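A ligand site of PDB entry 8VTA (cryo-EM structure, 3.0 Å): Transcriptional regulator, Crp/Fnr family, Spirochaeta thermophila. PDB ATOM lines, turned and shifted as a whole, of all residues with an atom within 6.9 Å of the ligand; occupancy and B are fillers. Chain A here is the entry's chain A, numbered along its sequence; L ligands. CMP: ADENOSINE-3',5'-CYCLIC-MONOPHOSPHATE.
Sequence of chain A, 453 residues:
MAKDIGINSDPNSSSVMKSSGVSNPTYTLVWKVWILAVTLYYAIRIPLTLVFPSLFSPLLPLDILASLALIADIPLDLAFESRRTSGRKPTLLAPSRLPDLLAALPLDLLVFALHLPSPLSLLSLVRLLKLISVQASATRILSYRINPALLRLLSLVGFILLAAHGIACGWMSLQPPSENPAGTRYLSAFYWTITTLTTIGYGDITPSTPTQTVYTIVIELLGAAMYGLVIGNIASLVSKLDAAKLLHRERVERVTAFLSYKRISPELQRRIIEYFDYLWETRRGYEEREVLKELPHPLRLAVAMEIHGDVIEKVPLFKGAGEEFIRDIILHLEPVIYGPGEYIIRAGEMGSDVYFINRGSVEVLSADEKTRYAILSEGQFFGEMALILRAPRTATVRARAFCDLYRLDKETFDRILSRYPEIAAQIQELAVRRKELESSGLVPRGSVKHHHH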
ATOM      1  N   ILE A 345       7.358  31.202  28.376  1.00  0.00           N
ATOM      2  CA  ILE A 345       7.442  30.018  29.237  1.00  0.00           C
ATOM      3  C   ILE A 345       8.493  29.089  28.655  1.00  0.00           C
ATOM      4  O   ILE A 345       8.569  28.912  27.432  1.00  0.00           O
ATOM      5  CB  ILE A 345       6.087  29.293  29.356  1.00  0.00           C
ATOM      6  CG1 ILE A 345       5.388  29.218  27.999  1.00  0.00           C
ATOM      7  CG2 ILE A 345       5.200  29.988  30.378  1.00  0.00           C
ATOM      8  CD1 ILE A 345       4.024  28.579  28.055  1.00  0.00           C
ATOM      9  N   ARG A 346       9.310  28.520  29.529  1.00  0.00           N
ATOM     10  CA  ARG A 346      10.346  27.577  29.116  1.00  0.00           C
ATOM     11  C   ARG A 346       9.851  26.156  29.336  1.00  0.00           C
ATOM     12  O   ARG A 346       9.004  25.891  30.189  1.00  0.00           O
ATOM     13  CB  ARG A 346      11.637  27.799  29.905  1.00  0.00           C
ATOM     14  CG  ARG A 346      12.353  29.099  29.582  1.00  0.00           C
ATOM     15  CD  ARG A 346      13.173  29.572  30.766  1.00  0.00           C
ATOM     16  NE  ARG A 346      12.350  30.233  31.773  1.00  0.00           N
ATOM     17  CZ  ARG A 346      12.253  31.548  31.930  1.00  0.00           C
ATOM     18  NH1 ARG A 346      12.933  32.381  31.165  1.00  0.00           N
ATOM     19  NH2 ARG A 346      11.457  32.034  32.879  1.00  0.00           N
ATOM     20  N   ASP A 353      -0.138  29.350  34.014  1.00  0.00           N
ATOM     21  CA  ASP A 353      -0.882  30.340  33.256  1.00  0.00           C
ATOM     22  C   ASP A 353      -1.006  29.907  31.809  1.00  0.00           C
ATOM     23  O   ASP A 353      -0.274  29.034  31.332  1.00  0.00           O
ATOM     24  CB  ASP A 353      -0.214  31.721  33.335  1.00  0.00           C
ATOM     25  CG  ASP A 353       1.294  31.636  33.362  1.00  0.00           C
ATOM     26  OD1 ASP A 353       1.832  30.512  33.309  1.00  0.00           O
ATOM     27  OD2 ASP A 353       1.952  32.699  33.420  1.00  0.00           O
ATOM     28  N   VAL A 364       7.244  28.446  19.249  1.00  0.00           N
ATOM     29  CA  VAL A 364       7.320  27.302  20.145  1.00  0.00           C
ATOM     30  C   VAL A 364       8.496  26.452  19.693  1.00  0.00           C
ATOM     31  O   VAL A 364       8.511  25.957  18.551  1.00  0.00           O
ATOM     32  CB  VAL A 364       6.020  26.503  20.149  1.00  0.00           C
ATOM     33  CG1 VAL A 364       6.091  25.405  21.180  1.00  0.00           C
ATOM     34  CG2 VAL A 364       4.855  27.420  20.424  1.00  0.00           C
ATOM     35  N   LEU A 365       9.477  26.281  20.580  1.00  0.00           N
ATOM     36  CA  LEU A 365      10.703  25.538  20.359  1.00  0.00           C
ATOM     37  C   LEU A 365      10.829  24.482  21.442  1.00  0.00           C
ATOM     38  O   LEU A 365       9.997  24.380  22.348  1.00  0.00           O
ATOM     39  CB  LEU A 365      11.931  26.467  20.382  1.00  0.00           C
ATOM     40  CG  LEU A 365      11.789  27.919  19.939  1.00  0.00           C
ATOM     41  CD1 LEU A 365      13.091  28.659  20.166  1.00  0.00           C
ATOM     42  CD2 LEU A 365      11.394  28.004  18.480  1.00  0.00           C
ATOM     43  N   TYR A 373       9.184  24.142  16.937  1.00  0.00           N
ATOM     44  CA  TYR A 373       7.957  23.356  16.780  1.00  0.00           C
ATOM     45  C   TYR A 373       6.932  24.111  15.958  1.00  0.00           C
ATOM     46  O   TYR A 373       6.329  23.551  15.038  1.00  0.00           O
ATOM     47  CB  TYR A 373       7.358  22.964  18.138  1.00  0.00           C
ATOM     48  CG  TYR A 373       8.186  22.064  19.054  1.00  0.00           C
ATOM     49  CD1 TYR A 373       9.561  21.909  18.891  1.00  0.00           C
ATOM     50  CD2 TYR A 373       7.569  21.356  20.076  1.00  0.00           C
ATOM     51  CE1 TYR A 373      10.285  21.081  19.730  1.00  0.00           C
ATOM     52  CE2 TYR A 373       8.288  20.541  20.916  1.00  0.00           C
ATOM     53  CZ  TYR A 373       9.648  20.405  20.735  1.00  0.00           C
ATOM     54  OH  TYR A 373      10.374  19.585  21.570  1.00  0.00           O
ATOM     55  N   ALA A 374       6.719  25.394  16.263  1.00  0.00           N
ATOM     56  CA  ALA A 374       5.643  26.134  15.613  1.00  0.00           C
ATOM     57  C   ALA A 374       5.887  27.628  15.710  1.00  0.00           C
ATOM     58  O   ALA A 374       6.756  28.085  16.462  1.00  0.00           O
ATOM     59  CB  ALA A 374       4.282  25.769  16.217  1.00  0.00           C
ATOM     60  N   ILE A 375       5.106  28.380  14.946  1.00  0.00           N
ATOM     61  CA  ILE A 375       5.058  29.832  15.008  1.00  0.00           C
ATOM     62  C   ILE A 375       3.599  30.233  15.204  1.00  0.00           C
ATOM     63  O   ILE A 375       2.736  29.828  14.422  1.00  0.00           O
ATOM     64  CB  ILE A 375       5.622  30.479  13.733  1.00  0.00           C
ATOM     65  CG1 ILE A 375       7.154  30.457  13.765  1.00  0.00           C
ATOM     66  CG2 ILE A 375       5.099  31.907  13.563  1.00  0.00           C
ATOM     67  CD1 ILE A 375       7.788  31.636  14.456  1.00  0.00           C
ATOM     68  N   LEU A 376       3.327  31.007  16.249  1.00  0.00           N
ATOM     69  CA  LEU A 376       1.965  31.395  16.604  1.00  0.00           C
ATOM     70  C   LEU A 376       1.840  32.914  16.595  1.00  0.00           C
ATOM     71  O   LEU A 376       2.652  33.605  17.210  1.00  0.00           O
ATOM     72  CB  LEU A 376       1.573  30.842  17.969  1.00  0.00           C
ATOM     73  CG  LEU A 376       2.067  29.453  18.344  1.00  0.00           C
ATOM     74  CD1 LEU A 376       1.724  29.167  19.789  1.00  0.00           C
ATOM     75  CD2 LEU A 376       1.477  28.404  17.436  1.00  0.00           C
ATOM     76  N   PHE A 381      -2.887  30.876  20.493  1.00  0.00           N
ATOM     77  CA  PHE A 381      -2.605  30.771  21.916  1.00  0.00           C
ATOM     78  C   PHE A 381      -1.592  29.664  22.160  1.00  0.00           C
ATOM     79  O   PHE A 381      -1.220  28.912  21.253  1.00  0.00           O
ATOM     80  CB  PHE A 381      -3.877  30.478  22.718  1.00  0.00           C
ATOM     81  CG  PHE A 381      -4.344  29.062  22.595  1.00  0.00           C
ATOM     82  CD1 PHE A 381      -4.634  28.501  21.356  1.00  0.00           C
ATOM     83  CD2 PHE A 381      -4.500  28.276  23.728  1.00  0.00           C
ATOM     84  CE1 PHE A 381      -5.066  27.198  21.257  1.00  0.00           C
ATOM     85  CE2 PHE A 381      -4.938  26.970  23.621  1.00  0.00           C
ATOM     86  CZ  PHE A 381      -5.211  26.431  22.391  1.00  0.00           C
ATOM     87  N   PHE A 382      -1.157  29.561  23.414  1.00  0.00           N
ATOM     88  CA  PHE A 382      -0.271  28.485  23.839  1.00  0.00           C
ATOM     89  C   PHE A 382      -0.356  28.339  25.349  1.00  0.00           C
ATOM     90  O   PHE A 382      -0.847  29.223  26.048  1.00  0.00           O
ATOM     91  CB  PHE A 382       1.175  28.746  23.411  1.00  0.00           C
ATOM     92  CG  PHE A 382       1.706  30.084  23.836  1.00  0.00           C
ATOM     93  CD1 PHE A 382       1.574  31.191  23.004  1.00  0.00           C
ATOM     94  CD2 PHE A 382       2.353  30.243  25.046  1.00  0.00           C
ATOM     95  CE1 PHE A 382       2.061  32.422  23.385  1.00  0.00           C
ATOM     96  CE2 PHE A 382       2.840  31.474  25.428  1.00  0.00           C
ATOM     97  CZ  PHE A 382       2.698  32.561  24.595  1.00  0.00           C
ATOM     98  N   GLY A 383       0.104  27.194  25.835  1.00  0.00           N
ATOM     99  CA  GLY A 383       0.158  26.946  27.261  1.00  0.00           C
ATOM    100  C   GLY A 383      -1.110  26.410  27.884  1.00  0.00           C
ATOM    101  O   GLY A 383      -1.314  26.590  29.090  1.00  0.00           O
ATOM    102  N   GLU A 384      -1.968  25.761  27.104  1.00  0.00           N
ATOM    103  CA  GLU A 384      -3.248  25.299  27.629  1.00  0.00           C
ATOM    104  C   GLU A 384      -3.132  24.003  28.428  1.00  0.00           C
ATOM    105  O   GLU A 384      -4.046  23.693  29.215  1.00  0.00           O
ATOM    106  CB  GLU A 384      -4.263  25.131  26.500  1.00  0.00           C
ATOM    107  CG  GLU A 384      -3.943  24.028  25.494  1.00  0.00           C
ATOM    108  CD  GLU A 384      -2.923  24.431  24.437  1.00  0.00           C
ATOM    109  OE1 GLU A 384      -2.148  25.389  24.660  1.00  0.00           O
ATOM    110  OE2 GLU A 384      -2.907  23.798  23.366  1.00  0.00           O
ATOM    111  N   MET A 385      -2.050  23.235  28.247  1.00  0.00           N
ATOM    112  CA  MET A 385      -1.854  22.034  29.052  1.00  0.00           C
ATOM    113  C   MET A 385      -1.804  22.379  30.537  1.00  0.00           C
ATOM    114  O   MET A 385      -2.471  21.745  31.362  1.00  0.00           O
ATOM    115  CB  MET A 385      -0.583  21.289  28.643  1.00  0.00           C
ATOM    116  CG  MET A 385      -0.066  21.574  27.244  1.00  0.00           C
ATOM    117  SD  MET A 385      -1.356  21.741  26.005  1.00  0.00           S
ATOM    118  CE  MET A 385      -1.995  20.070  25.944  1.00  0.00           C
ATOM    119  N   ALA A 386      -1.065  23.425  30.894  1.00  0.00           N
ATOM    120  CA  ALA A 386      -1.010  23.851  32.281  1.00  0.00           C
ATOM    121  C   ALA A 386      -2.352  24.333  32.792  1.00  0.00           C
ATOM    122  O   ALA A 386      -2.515  24.506  34.006  1.00  0.00           O
ATOM    123  CB  ALA A 386       0.046  24.954  32.459  1.00  0.00           C
ATOM    124  N   LEU A 387      -3.326  24.560  31.911  1.00  0.00           N
ATOM    125  CA  LEU A 387      -4.655  24.940  32.346  1.00  0.00           C
ATOM    126  C   LEU A 387      -5.495  23.760  32.802  1.00  0.00           C
ATOM    127  O   LEU A 387      -6.501  23.961  33.477  1.00  0.00           O
ATOM    128  CB  LEU A 387      -5.385  25.684  31.224  1.00  0.00           C
ATOM    129  CG  LEU A 387      -5.562  27.193  31.423  1.00  0.00           C
ATOM    130  CD1 LEU A 387      -6.755  27.697  30.622  1.00  0.00           C
ATOM    131  CD2 LEU A 387      -5.721  27.543  32.901  1.00  0.00           C
ATOM    132  N   LEU A 389      -3.679  20.625  33.830  1.00  0.00           N
ATOM    133  CA  LEU A 389      -2.806  19.784  34.648  1.00  0.00           C
ATOM    134  C   LEU A 389      -1.683  20.650  35.200  1.00  0.00           C
ATOM    135  O   LEU A 389      -1.417  21.740  34.694  1.00  0.00           O
ATOM    136  CB  LEU A 389      -2.268  18.582  33.856  1.00  0.00           C
ATOM    137  CG  LEU A 389      -1.742  18.705  32.423  1.00  0.00           C
ATOM    138  CD1 LEU A 389      -0.418  19.463  32.308  1.00  0.00           C
ATOM    139  CD2 LEU A 389      -1.623  17.329  31.788  1.00  0.00           C
ATOM    140  N   ALA A 391       1.457  19.435  35.360  1.00  0.00           N
ATOM    141  CA  ALA A 391       2.713  18.944  34.802  1.00  0.00           C
ATOM    142  C   ALA A 391       3.462  20.099  34.127  1.00  0.00           C
ATOM    143  O   ALA A 391       2.844  21.060  33.664  1.00  0.00           O
ATOM    144  CB  ALA A 391       2.443  17.823  33.805  1.00  0.00           C
ATOM    145  N   PRO A 392       4.792  20.023  34.071  1.00  0.00           N
ATOM    146  CA  PRO A 392       5.565  21.139  33.502  1.00  0.00           C
ATOM    147  C   PRO A 392       5.294  21.325  32.014  1.00  0.00           C
ATOM    148  O   PRO A 392       4.683  20.493  31.341  1.00  0.00           O
ATOM    149  CB  PRO A 392       7.019  20.725  33.749  1.00  0.00           C
ATOM    150  CG  PRO A 392       6.974  19.253  33.980  1.00  0.00           C
ATOM    151  CD  PRO A 392       5.667  19.011  34.669  1.00  0.00           C
ATOM    152  N   ARG A 393       5.751  22.471  31.515  1.00  0.00           N
ATOM    153  CA  ARG A 393       5.547  22.838  30.125  1.00  0.00           C
ATOM    154  C   ARG A 393       6.226  21.832  29.193  1.00  0.00           C
ATOM    155  O   ARG A 393       7.365  21.434  29.422  1.00  0.00           O
ATOM    156  CB  ARG A 393       6.092  24.238  29.859  1.00  0.00           C
ATOM    157  CG  ARG A 393       5.553  25.302  30.799  1.00  0.00           C
ATOM    158  CD  ARG A 393       4.123  25.679  30.478  1.00  0.00           C
ATOM    159  NE  ARG A 393       3.679  26.820  31.263  1.00  0.00           N
ATOM    160  CZ  ARG A 393       2.476  27.387  31.159  1.00  0.00           C
ATOM    161  NH1 ARG A 393       1.588  26.942  30.290  1.00  0.00           N
ATOM    162  NH2 ARG A 393       2.179  28.406  31.949  1.00  0.00           N
ATOM    163  N   THR A 394       5.510  21.444  28.140  1.00  0.00           N
ATOM    164  CA  THR A 394       6.057  20.493  27.181  1.00  0.00           C
ATOM    165  C   THR A 394       7.021  21.128  26.192  1.00  0.00           C
ATOM    166  O   THR A 394       7.758  20.407  25.521  1.00  0.00           O
ATOM    167  CB  THR A 394       4.924  19.796  26.417  1.00  0.00           C
ATOM    168  OG1 THR A 394       4.500  20.641  25.345  1.00  0.00           O
ATOM    169  CG2 THR A 394       3.748  19.533  27.344  1.00  0.00           C
ATOM    170  N   ALA A 395       7.023  22.454  26.091  1.00  0.00           N
ATOM    171  CA  ALA A 395       7.898  23.125  25.135  1.00  0.00           C
ATOM    172  C   ALA A 395       8.154  24.543  25.613  1.00  0.00           C
ATOM    173  O   ALA A 395       7.438  25.079  26.464  1.00  0.00           O
ATOM    174  CB  ALA A 395       7.289  23.131  23.731  1.00  0.00           C
ATOM    175  N   THR A 396       9.208  25.145  25.048  1.00  0.00           N
ATOM    176  CA  THR A 396       9.583  26.512  25.370  1.00  0.00           C
ATOM    177  C   THR A 396       8.915  27.454  24.385  1.00  0.00           C
ATOM    178  O   THR A 396       8.779  27.146  23.201  1.00  0.00           O
ATOM    179  CB  THR A 396      11.109  26.671  25.326  1.00  0.00           C
ATOM    180  OG1 THR A 396      11.705  25.807  26.297  1.00  0.00           O
ATOM    181  CG2 THR A 396      11.529  28.105  25.623  1.00  0.00           C
ATOM    182  N   VAL A 397       8.470  28.615  24.870  1.00  0.00           N
ATOM    183  CA  VAL A 397       7.864  29.639  24.037  1.00  0.00           C
ATOM    184  C   VAL A 397       8.730  30.881  24.112  1.00  0.00           C
ATOM    185  O   VAL A 397       8.994  31.406  25.199  1.00  0.00           O
ATOM    186  CB  VAL A 397       6.423  29.942  24.460  1.00  0.00           C
ATOM    187  CG1 VAL A 397       5.853  31.039  23.582  1.00  0.00           C
ATOM    188  CG2 VAL A 397       5.567  28.691  24.367  1.00  0.00           C
HETATM  189  P   CMP L   1       2.573  23.972  26.856  1.00  0.00           P
HETATM  190  O1P CMP L   1       3.299  22.709  26.665  1.00  0.00           O
HETATM  191  O2P CMP L   1       1.952  24.275  28.162  1.00  0.00           O
HETATM  192  O5' CMP L   1       3.604  25.160  26.508  1.00  0.00           O
HETATM  193  C5' CMP L   1       4.071  25.364  25.179  1.00  0.00           C
HETATM  194  C4' CMP L   1       2.882  25.372  24.283  1.00  0.00           C
HETATM  195  O4' CMP L   1       3.201  25.367  22.873  1.00  0.00           O
HETATM  196  C3' CMP L   1       2.046  24.138  24.428  1.00  0.00           C
HETATM  197  O3' CMP L   1       1.447  24.091  25.707  1.00  0.00           O
HETATM  198  C2' CMP L   1       1.122  24.262  23.225  1.00  0.00           C
HETATM  199  O2' CMP L   1       0.150  25.265  23.447  1.00  0.00           O
HETATM  200  C1' CMP L   1       2.112  24.798  22.174  1.00  0.00           C
HETATM  201  N9  CMP L   1       2.614  23.738  21.275  1.00  0.00           N
HETATM  202  C8  CMP L   1       3.566  22.795  21.554  1.00  0.00           C
HETATM  203  N7  CMP L   1       3.810  21.990  20.552  1.00  0.00           N
HETATM  204  C5  CMP L   1       2.970  22.432  19.544  1.00  0.00           C
HETATM  205  C6  CMP L   1       2.755  21.995  18.221  1.00  0.00           C
HETATM  206  N6  CMP L   1       3.402  20.970  17.676  1.00  0.00           N
HETATM  207  N1  CMP L   1       1.846  22.667  17.483  1.00  0.00           N
HETATM  208  C2  CMP L   1       1.204  23.693  18.035  1.00  0.00           C
HETATM  209  N3  CMP L   1       1.325  24.192  19.264  1.00  0.00           N
HETATM  210  C4  CMP L   1       2.232  23.521  19.977  1.00  0.00           C
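The backbone NH of Val 397 is in hydrogen-bond range of the backbone carbonyl oxygen of Ile 345 (2.6 Å). O of Gly 383 is in hydrogen-bond range of NH1 of Arg 393, 3.2 Å away. The backbone NH of Val 364 is in hydrogen-bond range of the backbone carbonyl oxygen of Ala 374 (2.9 Å). The guanidinium group (NH2) of Arg 393 is in salt-bridge range of the side-chain carboxylate (OD1) of Asp 353 (2.5 Å). O of Val 364 is in hydrogen-bond range of N of Tyr 373, at 2.5 Å.
An oxygen (O3') of the ligand sits close to the side-chain sulfur (SD) of Met 385 (3.7 Å). CD1 of Ile 345 touches O5' of the ligand, 3.8 Å away. CG1 of Val 364 touches O4' of the ligand (3.3 Å). CD2 of Tyr 373 touches N7 of the ligand, at 3.8 Å. CA of Phe 382 touches O2' of the ligand, at 3.3 Å. Ala 395 touches the ligand. CG2 of Val 397 touches C5' of the ligand, at 3.7 Å. Within 4 Å of the ligand: Ile 345, Val 364, Tyr 373, Phe 382, Gly 383, Glu 384, Met 385, Arg 393, Thr 394, Ala 395 and Val 397.
O1P of the ligand lies within hydrogen-bond range of OG1 of Thr 394, at 2.7 Å. The backbone NH (N) of Gly 383 is in hydrogen-bond range of an oxygen (O2') of the ligand, 3.1 Å away. The guanidinium group (NH1) of Arg 393 is in salt-bridge range of an oxygen (O2P) of the ligand (3.4 Å). The side-chain carboxylate of Glu 384 sits at hydrogen-bond distance from an oxygen (O2') of the ligand. The backbone NH (N) of Thr 394 is in hydrogen-bond range of an oxygen (O1P) of the ligand, 2.9 Å away.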
